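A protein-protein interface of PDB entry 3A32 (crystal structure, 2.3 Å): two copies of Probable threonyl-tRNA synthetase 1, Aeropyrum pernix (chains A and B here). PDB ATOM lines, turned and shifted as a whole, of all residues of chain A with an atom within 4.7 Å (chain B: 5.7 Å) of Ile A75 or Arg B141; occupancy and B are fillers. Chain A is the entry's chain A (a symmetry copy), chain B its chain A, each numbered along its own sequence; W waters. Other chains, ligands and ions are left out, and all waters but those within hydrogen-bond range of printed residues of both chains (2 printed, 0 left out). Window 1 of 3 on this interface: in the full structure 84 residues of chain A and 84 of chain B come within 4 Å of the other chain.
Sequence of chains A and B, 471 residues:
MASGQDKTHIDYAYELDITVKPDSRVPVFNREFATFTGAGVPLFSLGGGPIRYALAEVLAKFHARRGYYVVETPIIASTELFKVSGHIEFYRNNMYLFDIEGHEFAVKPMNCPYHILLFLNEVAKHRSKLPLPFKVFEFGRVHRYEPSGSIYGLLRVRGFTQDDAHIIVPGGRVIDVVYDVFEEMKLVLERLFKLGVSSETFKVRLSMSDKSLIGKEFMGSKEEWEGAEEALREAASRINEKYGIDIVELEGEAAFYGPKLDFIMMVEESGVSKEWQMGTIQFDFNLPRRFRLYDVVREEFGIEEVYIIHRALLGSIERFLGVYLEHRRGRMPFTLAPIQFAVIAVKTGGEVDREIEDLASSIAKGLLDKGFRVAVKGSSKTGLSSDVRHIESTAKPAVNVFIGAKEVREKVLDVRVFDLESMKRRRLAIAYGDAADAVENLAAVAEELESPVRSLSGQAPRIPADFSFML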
ATOM      1  N   GLU A  72       6.336  -8.550  22.393  1.00  0.00           N
ATOM      2  CA  GLU A  72       7.388  -8.670  21.381  1.00  0.00           C
ATOM      3  C   GLU A  72       8.588  -9.258  22.140  1.00  0.00           C
ATOM      4  O   GLU A  72       8.960  -8.750  23.228  1.00  0.00           O
ATOM      5  CB  GLU A  72       7.684  -7.316  20.724  1.00  0.00           C
ATOM      6  CG  GLU A  72       8.987  -7.312  19.895  1.00  0.00           C
ATOM      7  CD  GLU A  72       9.162  -6.086  18.946  1.00  0.00           C
ATOM      8  OE1 GLU A  72       8.290  -5.190  18.962  1.00  0.00           O
ATOM      9  OE2 GLU A  72      10.176  -6.063  18.144  1.00  0.00           O
ATOM     10  N   THR A  73       9.134 -10.362  21.621  1.00  0.00           N
ATOM     11  CA  THR A  73      10.234 -11.048  22.329  1.00  0.00           C
ATOM     12  C   THR A  73      11.500 -10.980  21.470  1.00  0.00           C
ATOM     13  O   THR A  73      11.403 -10.771  20.255  1.00  0.00           O
ATOM     14  CB  THR A  73       9.845 -12.518  22.797  1.00  0.00           C
ATOM     15  OG1 THR A  73       9.529 -13.355  21.666  1.00  0.00           O
ATOM     16  CG2 THR A  73       8.650 -12.515  23.812  1.00  0.00           C
ATOM     17  N   PRO A  74      12.691 -11.147  22.085  1.00  0.00           N
ATOM     18  CA  PRO A  74      13.905 -10.980  21.299  1.00  0.00           C
ATOM     19  C   PRO A  74      14.065 -11.886  20.112  1.00  0.00           C
ATOM     20  O   PRO A  74      13.505 -12.996  20.051  1.00  0.00           O
ATOM     21  CB  PRO A  74      15.015 -11.251  22.299  1.00  0.00           C
ATOM     22  CG  PRO A  74      14.387 -10.898  23.621  1.00  0.00           C
ATOM     23  CD  PRO A  74      12.997 -11.426  23.489  1.00  0.00           C
ATOM     24  N   ILE A  75      14.843 -11.400  19.156  1.00  0.00           N
ATOM     25  CA  ILE A  75      15.154 -12.163  17.983  1.00  0.00           C
ATOM     26  C   ILE A  75      16.253 -13.213  18.176  1.00  0.00           C
ATOM     27  O   ILE A  75      16.255 -14.237  17.444  1.00  0.00           O
ATOM     28  CB  ILE A  75      15.365 -11.202  16.793  1.00  0.00           C
ATOM     29  CG1 ILE A  75      13.974 -10.609  16.523  1.00  0.00           C
ATOM     30  CG2 ILE A  75      16.042 -11.931  15.573  1.00  0.00           C
ATOM     31  CD1 ILE A  75      13.769  -9.917  15.244  1.00  0.00           C
ATOM     32  N   ILE A  76      17.157 -12.987  19.140  1.00  0.00           N
ATOM     33  CA  ILE A  76      18.217 -13.940  19.430  1.00  0.00           C
ATOM     34  C   ILE A  76      18.082 -14.448  20.858  1.00  0.00           C
ATOM     35  O   ILE A  76      17.324 -13.890  21.648  1.00  0.00           O
ATOM     36  CB  ILE A  76      19.603 -13.391  19.135  1.00  0.00           C
ATOM     37  CG1 ILE A  76      19.955 -12.181  20.056  1.00  0.00           C
ATOM     38  CG2 ILE A  76      19.719 -13.079  17.628  1.00  0.00           C
ATOM     39  CD1 ILE A  76      21.537 -11.765  20.082  1.00  0.00           C
ATOM     40  N   ALA A  77      18.744 -15.547  21.163  1.00  0.00           N
ATOM     41  CA  ALA A  77      18.711 -16.088  22.513  1.00  0.00           C
ATOM     42  C   ALA A  77      19.903 -16.991  22.705  1.00  0.00           C
ATOM     43  O   ALA A  77      20.366 -17.596  21.749  1.00  0.00           O
ATOM     44  CB  ALA A  77      17.421 -16.893  22.772  1.00  0.00           C
ATOM     45  N   ALA A 106      21.423 -18.508  19.212  1.00  0.00           N
ATOM     46  CA  ALA A 106      20.646 -18.873  18.065  1.00  0.00           C
ATOM     47  C   ALA A 106      19.761 -17.691  17.666  1.00  0.00           C
ATOM     48  O   ALA A 106      19.306 -16.924  18.522  1.00  0.00           O
ATOM     49  CB  ALA A 106      19.748 -20.068  18.408  1.00  0.00           C
ATOM     50  N   VAL A 107      19.499 -17.578  16.365  1.00  0.00           N
ATOM     51  CA  VAL A 107      18.410 -16.787  15.870  1.00  0.00           C
ATOM     52  C   VAL A 107      17.162 -17.606  16.205  1.00  0.00           C
ATOM     53  O   VAL A 107      17.087 -18.832  15.922  1.00  0.00           O
ATOM     54  CB  VAL A 107      18.572 -16.526  14.342  1.00  0.00           C
ATOM     55  CG1 VAL A 107      17.504 -15.587  13.830  1.00  0.00           C
ATOM     56  CG2 VAL A 107      19.990 -15.924  14.070  1.00  0.00           C
ATOM     57  N   LYS A 108      16.216 -16.951  16.874  1.00  0.00           N
ATOM     58  CA  LYS A 108      14.989 -17.561  17.364  1.00  0.00           C
ATOM     59  C   LYS A 108      14.255 -18.295  16.235  1.00  0.00           C
ATOM     60  O   LYS A 108      13.927 -17.678  15.197  1.00  0.00           O
ATOM     61  CB  LYS A 108      14.105 -16.435  17.912  1.00  0.00           C
ATOM     62  CG  LYS A 108      12.777 -16.810  18.468  1.00  0.00           C
ATOM     63  CD  LYS A 108      12.037 -15.599  19.075  1.00  0.00           C
ATOM     64  CE  LYS A 108      11.577 -14.592  18.019  1.00  0.00           C
ATOM     65  NZ  LYS A 108      10.773 -13.533  18.717  1.00  0.00           N
ATOM     66  N   ARG A 141       8.788 -13.005  14.685  1.00  0.00           N
ATOM     67  CA  ARG A 141       9.719 -13.202  13.528  1.00  0.00           C
ATOM     68  C   ARG A 141      10.700 -14.328  13.828  1.00  0.00           C
ATOM     69  O   ARG A 141      11.485 -14.227  14.772  1.00  0.00           O
ATOM     70  CB  ARG A 141      10.486 -11.923  13.229  1.00  0.00           C
ATOM     71  CG  ARG A 141       9.554 -10.782  12.856  1.00  0.00           C
ATOM     72  CD  ARG A 141      10.176  -9.429  13.084  1.00  0.00           C
ATOM     73  NE  ARG A 141       9.354  -8.439  12.390  1.00  0.00           N
ATOM     74  CZ  ARG A 141       8.401  -7.756  13.000  1.00  0.00           C
ATOM     75  NH1 ARG A 141       8.210  -7.930  14.303  1.00  0.00           N
ATOM     76  NH2 ARG A 141       7.660  -6.924  12.313  1.00  0.00           N
ATOM     77  N   VAL B  41      20.395  -8.818  25.954  1.00  0.00           N
ATOM     78  CA  VAL B  41      19.237  -9.088  25.097  1.00  0.00           C
ATOM     79  C   VAL B  41      17.948  -8.701  25.848  1.00  0.00           C
ATOM     80  O   VAL B  41      17.360  -9.531  26.563  1.00  0.00           O
ATOM     81  CB  VAL B  41      19.158 -10.580  24.679  1.00  0.00           C
ATOM     82  CG1 VAL B  41      18.022 -10.805  23.679  1.00  0.00           C
ATOM     83  CG2 VAL B  41      20.516 -11.034  24.071  1.00  0.00           C
ATOM     84  N   ARG B  52       5.777  -1.172  22.575  1.00  0.00           N
ATOM     85  CA  ARG B  52       6.481  -1.483  21.330  1.00  0.00           C
ATOM     86  C   ARG B  52       5.588  -1.443  20.089  1.00  0.00           C
ATOM     87  O   ARG B  52       5.981  -0.885  19.081  1.00  0.00           O
ATOM     88  CB  ARG B  52       7.246  -2.809  21.448  1.00  0.00           C
ATOM     89  CG  ARG B  52       8.510  -2.584  22.381  1.00  0.00           C
ATOM     90  CD  ARG B  52       9.427  -3.786  22.343  1.00  0.00           C
ATOM     91  NE  ARG B  52      10.051  -3.959  21.030  1.00  0.00           N
ATOM     92  CZ  ARG B  52      11.145  -3.297  20.623  1.00  0.00           C
ATOM     93  NH1 ARG B  52      11.743  -2.420  21.425  1.00  0.00           N
ATOM     94  NH2 ARG B  52      11.661  -3.535  19.429  1.00  0.00           N
ATOM     95  N   ALA B  56       5.935   1.534  17.061  1.00  0.00           N
ATOM     96  CA  ALA B  56       6.092   1.208  15.648  1.00  0.00           C
ATOM     97  C   ALA B  56       5.048   1.899  14.788  1.00  0.00           C
ATOM     98  O   ALA B  56       5.357   2.416  13.709  1.00  0.00           O
ATOM     99  CB  ALA B  56       6.005  -0.330  15.417  1.00  0.00           C
ATOM    100  N   GLU B  72       9.736  -2.645   5.794  1.00  0.00           N
ATOM    101  CA  GLU B  72      10.286  -3.610   6.747  1.00  0.00           C
ATOM    102  C   GLU B  72      11.236  -4.481   5.911  1.00  0.00           C
ATOM    103  O   GLU B  72      10.848  -4.977   4.823  1.00  0.00           O
ATOM    104  CB  GLU B  72       9.172  -4.410   7.435  1.00  0.00           C
ATOM    105  CG  GLU B  72       9.690  -5.648   8.197  1.00  0.00           C
ATOM    106  CD  GLU B  72       8.663  -6.298   9.177  1.00  0.00           C
ATOM    107  OE1 GLU B  72       7.509  -5.820   9.235  1.00  0.00           O
ATOM    108  OE2 GLU B  72       9.056  -7.274   9.928  1.00  0.00           O
ATOM    109  N   ILE B  75      15.682  -9.591   8.505  1.00  0.00           N
ATOM    110  CA  ILE B  75      16.563  -9.637   9.635  1.00  0.00           C
ATOM    111  C   ILE B  75      17.934 -10.260   9.353  1.00  0.00           C
ATOM    112  O   ILE B  75      18.921  -9.907  10.048  1.00  0.00           O
ATOM    113  CB  ILE B  75      15.808 -10.229  10.845  1.00  0.00           C
ATOM    114  CG1 ILE B  75      14.758  -9.167  11.204  1.00  0.00           C
ATOM    115  CG2 ILE B  75      16.796 -10.628  12.004  1.00  0.00           C
ATOM    116  CD1 ILE B  75      14.103  -9.276  12.514  1.00  0.00           C
ATOM    117  N   VAL B 107      23.273 -11.715  10.852  1.00  0.00           N
ATOM    118  CA  VAL B 107      22.162 -11.014  11.426  1.00  0.00           C
ATOM    119  C   VAL B 107      22.444  -9.541  11.127  1.00  0.00           C
ATOM    120  O   VAL B 107      23.568  -9.026  11.372  1.00  0.00           O
ATOM    121  CB  VAL B 107      22.055 -11.313  12.952  1.00  0.00           C
ATOM    122  CG1 VAL B 107      20.815 -10.687  13.549  1.00  0.00           C
ATOM    123  CG2 VAL B 107      22.033 -12.862  13.174  1.00  0.00           C
ATOM    124  N   LYS B 108      21.454  -8.884  10.527  1.00  0.00           N
ATOM    125  CA  LYS B 108      21.542  -7.502  10.079  1.00  0.00           C
ATOM    126  C   LYS B 108      22.009  -6.587  11.218  1.00  0.00           C
ATOM    127  O   LYS B 108      21.367  -6.546  12.291  1.00  0.00           O
ATOM    128  CB  LYS B 108      20.144  -7.081   9.614  1.00  0.00           C
ATOM    129  CG  LYS B 108      19.974  -5.691   9.113  1.00  0.00           C
ATOM    130  CD  LYS B 108      18.547  -5.432   8.585  1.00  0.00           C
ATOM    131  CE  LYS B 108      17.496  -5.415   9.695  1.00  0.00           C
ATOM    132  NZ  LYS B 108      16.181  -5.037   9.074  1.00  0.00           N
ATOM    133  N   ASN B 111      20.230  -1.236   8.555  1.00  0.00           N
ATOM    134  CA  ASN B 111      19.174  -1.381   7.500  1.00  0.00           C
ATOM    135  C   ASN B 111      19.552  -0.787   6.170  1.00  0.00           C
ATOM    136  O   ASN B 111      18.934  -1.111   5.148  1.00  0.00           O
ATOM    137  CB  ASN B 111      17.846  -0.761   7.906  1.00  0.00           C
ATOM    138  CG  ASN B 111      17.385  -1.195   9.273  1.00  0.00           C
ATOM    139  OD1 ASN B 111      17.222  -0.378  10.182  1.00  0.00           O
ATOM    140  ND2 ASN B 111      17.159  -2.464   9.432  1.00  0.00           N
ATOM    141  N   GLU B 138      12.070   2.953   8.395  1.00  0.00           N
ATOM    142  CA  GLU B 138      11.851   1.602   8.955  1.00  0.00           C
ATOM    143  C   GLU B 138      12.033   1.614  10.462  1.00  0.00           C
ATOM    144  O   GLU B 138      13.011   2.187  10.933  1.00  0.00           O
ATOM    145  CB  GLU B 138      12.776   0.531   8.336  1.00  0.00           C
ATOM    146  CG  GLU B 138      12.620  -0.822   8.994  1.00  0.00           C
ATOM    147  CD  GLU B 138      13.307  -1.967   8.256  1.00  0.00           C
ATOM    148  OE1 GLU B 138      14.033  -1.741   7.242  1.00  0.00           O
ATOM    149  OE2 GLU B 138      13.139  -3.119   8.714  1.00  0.00           O
ATOM    150  N   PHE B 139      11.057   1.043  11.189  1.00  0.00           N
ATOM    151  CA  PHE B 139      11.182   0.694  12.617  1.00  0.00           C
ATOM    152  C   PHE B 139      12.037  -0.573  12.601  1.00  0.00           C
ATOM    153  O   PHE B 139      11.523  -1.698  12.470  1.00  0.00           O
ATOM    154  CB  PHE B 139       9.776   0.405  13.182  1.00  0.00           C
ATOM    155  CG  PHE B 139       9.712   0.289  14.702  1.00  0.00           C
ATOM    156  CD1 PHE B 139       9.791   1.418  15.515  1.00  0.00           C
ATOM    157  CD2 PHE B 139       9.530  -0.951  15.311  1.00  0.00           C
ATOM    158  CE1 PHE B 139       9.738   1.298  16.929  1.00  0.00           C
ATOM    159  CE2 PHE B 139       9.437  -1.074  16.698  1.00  0.00           C
ATOM    160  CZ  PHE B 139       9.537   0.058  17.510  1.00  0.00           C
ATOM    161  N   GLY B 140      13.355  -0.411  12.652  1.00  0.00           N
ATOM    162  CA  GLY B 140      14.231  -1.524  12.214  1.00  0.00           C
ATOM    163  C   GLY B 140      14.905  -2.233  13.359  1.00  0.00           C
ATOM    164  O   GLY B 140      15.224  -1.598  14.357  1.00  0.00           O
ATOM    165  N   ARG B 141      15.159  -3.528  13.215  1.00  0.00           N
ATOM    166  CA  ARG B 141      15.743  -4.358  14.317  1.00  0.00           C
ATOM    167  C   ARG B 141      17.135  -4.840  13.931  1.00  0.00           C
ATOM    168  O   ARG B 141      17.284  -5.574  12.953  1.00  0.00           O
ATOM    169  CB  ARG B 141      14.854  -5.554  14.621  1.00  0.00           C
ATOM    170  CG  ARG B 141      13.470  -5.124  15.078  1.00  0.00           C
ATOM    171  CD  ARG B 141      12.432  -6.196  14.865  1.00  0.00           C
ATOM    172  NE  ARG B 141      11.245  -5.824  15.633  1.00  0.00           N
ATOM    173  CZ  ARG B 141      10.228  -5.173  15.094  1.00  0.00           C
ATOM    174  NH1 ARG B 141      10.254  -4.887  13.797  1.00  0.00           N
ATOM    175  NH2 ARG B 141       9.217  -4.817  15.845  1.00  0.00           N
ATOM    176  N   VAL B 142      18.137  -4.385  14.690  1.00  0.00           N
ATOM    177  CA  VAL B 142      19.536  -4.543  14.351  1.00  0.00           C
ATOM    178  C   VAL B 142      20.281  -5.239  15.475  1.00  0.00           C
ATOM    179  O   VAL B 142      19.897  -5.159  16.638  1.00  0.00           O
ATOM    180  CB  VAL B 142      20.203  -3.199  13.898  1.00  0.00           C
ATOM    181  CG1 VAL B 142      19.529  -2.656  12.621  1.00  0.00           C
ATOM    182  CG2 VAL B 142      20.175  -2.138  14.981  1.00  0.00           C
ATOM    183  N   HIS B 143      21.297  -6.003  15.124  1.00  0.00           N
ATOM    184  CA  HIS B 143      22.018  -6.766  16.117  1.00  0.00           C
ATOM    185  C   HIS B 143      23.507  -6.584  15.869  1.00  0.00           C
ATOM    186  O   HIS B 143      23.961  -6.652  14.731  1.00  0.00           O
ATOM    187  CB  HIS B 143      21.694  -8.246  16.057  1.00  0.00           C
ATOM    188  CG  HIS B 143      20.298  -8.557  16.443  1.00  0.00           C
ATOM    189  ND1 HIS B 143      19.233  -8.413  15.567  1.00  0.00           N
ATOM    190  CD2 HIS B 143      19.781  -8.985  17.609  1.00  0.00           C
ATOM    191  CE1 HIS B 143      18.117  -8.731  16.196  1.00  0.00           C
ATOM    192  NE2 HIS B 143      18.419  -9.050  17.441  1.00  0.00           N
ATOM    193  N   PHE B 160      18.601  -4.198  19.171  1.00  0.00           N
ATOM    194  CA  PHE B 160      17.832  -3.014  19.470  1.00  0.00           C
ATOM    195  C   PHE B 160      17.085  -2.495  18.236  1.00  0.00           C
ATOM    196  O   PHE B 160      17.222  -3.026  17.148  1.00  0.00           O
ATOM    197  CB  PHE B 160      18.721  -1.880  20.127  1.00  0.00           C
ATOM    198  CG  PHE B 160      19.900  -1.434  19.284  1.00  0.00           C
ATOM    199  CD1 PHE B 160      19.831  -0.263  18.526  1.00  0.00           C
ATOM    200  CD2 PHE B 160      21.072  -2.204  19.225  1.00  0.00           C
ATOM    201  CE1 PHE B 160      20.907   0.148  17.692  1.00  0.00           C
ATOM    202  CE2 PHE B 160      22.165  -1.784  18.420  1.00  0.00           C
ATOM    203  CZ  PHE B 160      22.073  -0.614  17.640  1.00  0.00           C
ATOM    204  N   THR B 161      16.326  -1.423  18.432  1.00  0.00           N
ATOM    205  CA  THR B 161      15.466  -0.874  17.412  1.00  0.00           C
ATOM    206  C   THR B 161      15.882   0.576  17.141  1.00  0.00           C
ATOM    207  O   THR B 161      16.245   1.282  18.068  1.00  0.00           O
ATOM    208  CB  THR B 161      13.987  -1.055  17.855  1.00  0.00           C
ATOM    209  OG1 THR B 161      13.851  -2.315  18.576  1.00  0.00           O
ATOM    210  CG2 THR B 161      13.034  -1.057  16.618  1.00  0.00           C
ATOM    211  N   GLN B 162      15.841   0.993  15.876  1.00  0.00           N
ATOM    212  CA  GLN B 162      16.152   2.371  15.434  1.00  0.00           C
ATOM    213  C   GLN B 162      14.916   2.872  14.680  1.00  0.00           C
ATOM    214  O   GLN B 162      14.271   2.083  14.010  1.00  0.00           O
ATOM    215  CB  GLN B 162      17.270   2.354  14.398  1.00  0.00           C
ATOM    216  CG  GLN B 162      18.616   1.931  14.895  1.00  0.00           C
ATOM    217  CD  GLN B 162      19.554   1.507  13.802  1.00  0.00           C
ATOM    218  OE1 GLN B 162      19.168   0.871  12.827  1.00  0.00           O
ATOM    219  NE2 GLN B 162      20.819   1.845  13.968  1.00  0.00           N
HETATM  220  O   HOH W   1       6.183  -3.307  17.038  1.00  0.00           O
HETATM  221  O   HOH W   2      16.637  -9.367  19.529  1.00  0.00           O
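NE of Arg A141 lies within salt-bridge range of OE2 of Glu B72, at 2.7 Å. OE2 of Glu A72 lies within salt-bridge range of NE of Arg B141 (2.7 Å). The side-chain carboxylate (OE1) of Glu A72 is in salt-bridge range of the guanidinium group (NE) of Arg B52.
The backbone carbonyl oxygen (O) of Lys B108 lies within hydrogen-bond range of the backbone NH (N) of His B143, at 2.9 Å. The backbone carbonyl oxygen (O) of Ile A75 lies within hydrogen-bond range of the backbone NH (N) of Lys A108 (2.8 Å). OG1 of Thr B161 lies within hydrogen-bond range of NH2 of Arg B52 (2.6 Å). The backbone carbonyl oxygen (O) of Pro A74 is in hydrogen-bond range of the side-chain amino group (NZ) of Lys A108, 3.1 Å away. The backbone carbonyl oxygen (O) of Ile B75 sits at hydrogen-bond distance from the backbone NH (N) of Lys B108, 2.8 Å away.
CB of Pro A74 touches CG1 of Val B41, at 3.3 Å. CD1 of Ile A75 touches CD1 of Ile B75, 2.8 Å away. Arg B141 touches Ile A75 (CD to CD1, 3.97 Å). Ile A75 touches His B143 (CB to CE1, 3.7 Å). Val B41 touches Ile A76. Val A107 touches Val B107 (CG2 to CG2, 3.8 Å). Arg A141 touches Ile B75. Arg A141 touches Arg B141 (NH1 to CZ, 3.5 Å).
Of the printed residues of chain B, Ile A75 touches Ile B75, Arg B141 and His B143. Of chain A, only Glu A72 (2.7 Å), Ile A75 (3.97 Å) and Arg A141 (3.5 Å) come within 4 Å of Arg B141. Of the printed residues of chain A, Val B107 touches Val A107 (3.8 Å). Printed residues of chain A within 4 Å of Ile B75: Ile A75 and Arg A141. Of the printed residues of chain B, Glu A72 touches Arg B52 (3.0 Å) and Arg B141 (2.7 Å). Thr A73 touches none of the printed residues of chain B. The nearest residue of chain B that does not touch Ile A75 is Val B107 (5.3 Å). The nearest printed residue of chain A that does not touch Arg B141 is Thr A73 (6.8 Å). The nearest printed residue of chain A that does not touch Val B107 is Ile A76 (4.9 Å).
Of the 17 printed residues of chain B, 7 touch a printed residue of chain A. Hydrophobic or aromatic side chains of chain B within 4 Å of the printed part of chain A: Val B41, Ile B75, Val B107 and His B143. Hydrophobic or aromatic side chains of chain A within 4 Å of the printed part of chain B: Pro A74, Ile A75 and Val A107. Among the printed residues, 11 pairs touch across the chains.
Glu A72 touches Arg B141, and with the chains exchanged Arg A141 touches Glu B72. Ile B75 touches its own counterpart, Ile A75. Ile A75 touches Arg B141, and with the chains exchanged Arg A141 touches Ile B75. Arg A141 touches its own counterpart, Arg B141. 5 positions are printed for both chains.
Water W2 lies within hydrogen-bond range of the backbone NH (N) of Ile A75 (2.7 Å) and a ring nitrogen (NE2) of His B143 (2.8 Å). Water W1 bridges O of Arg B52 (3.2 Å) and OE1 of Glu A72 (3.4 Å).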
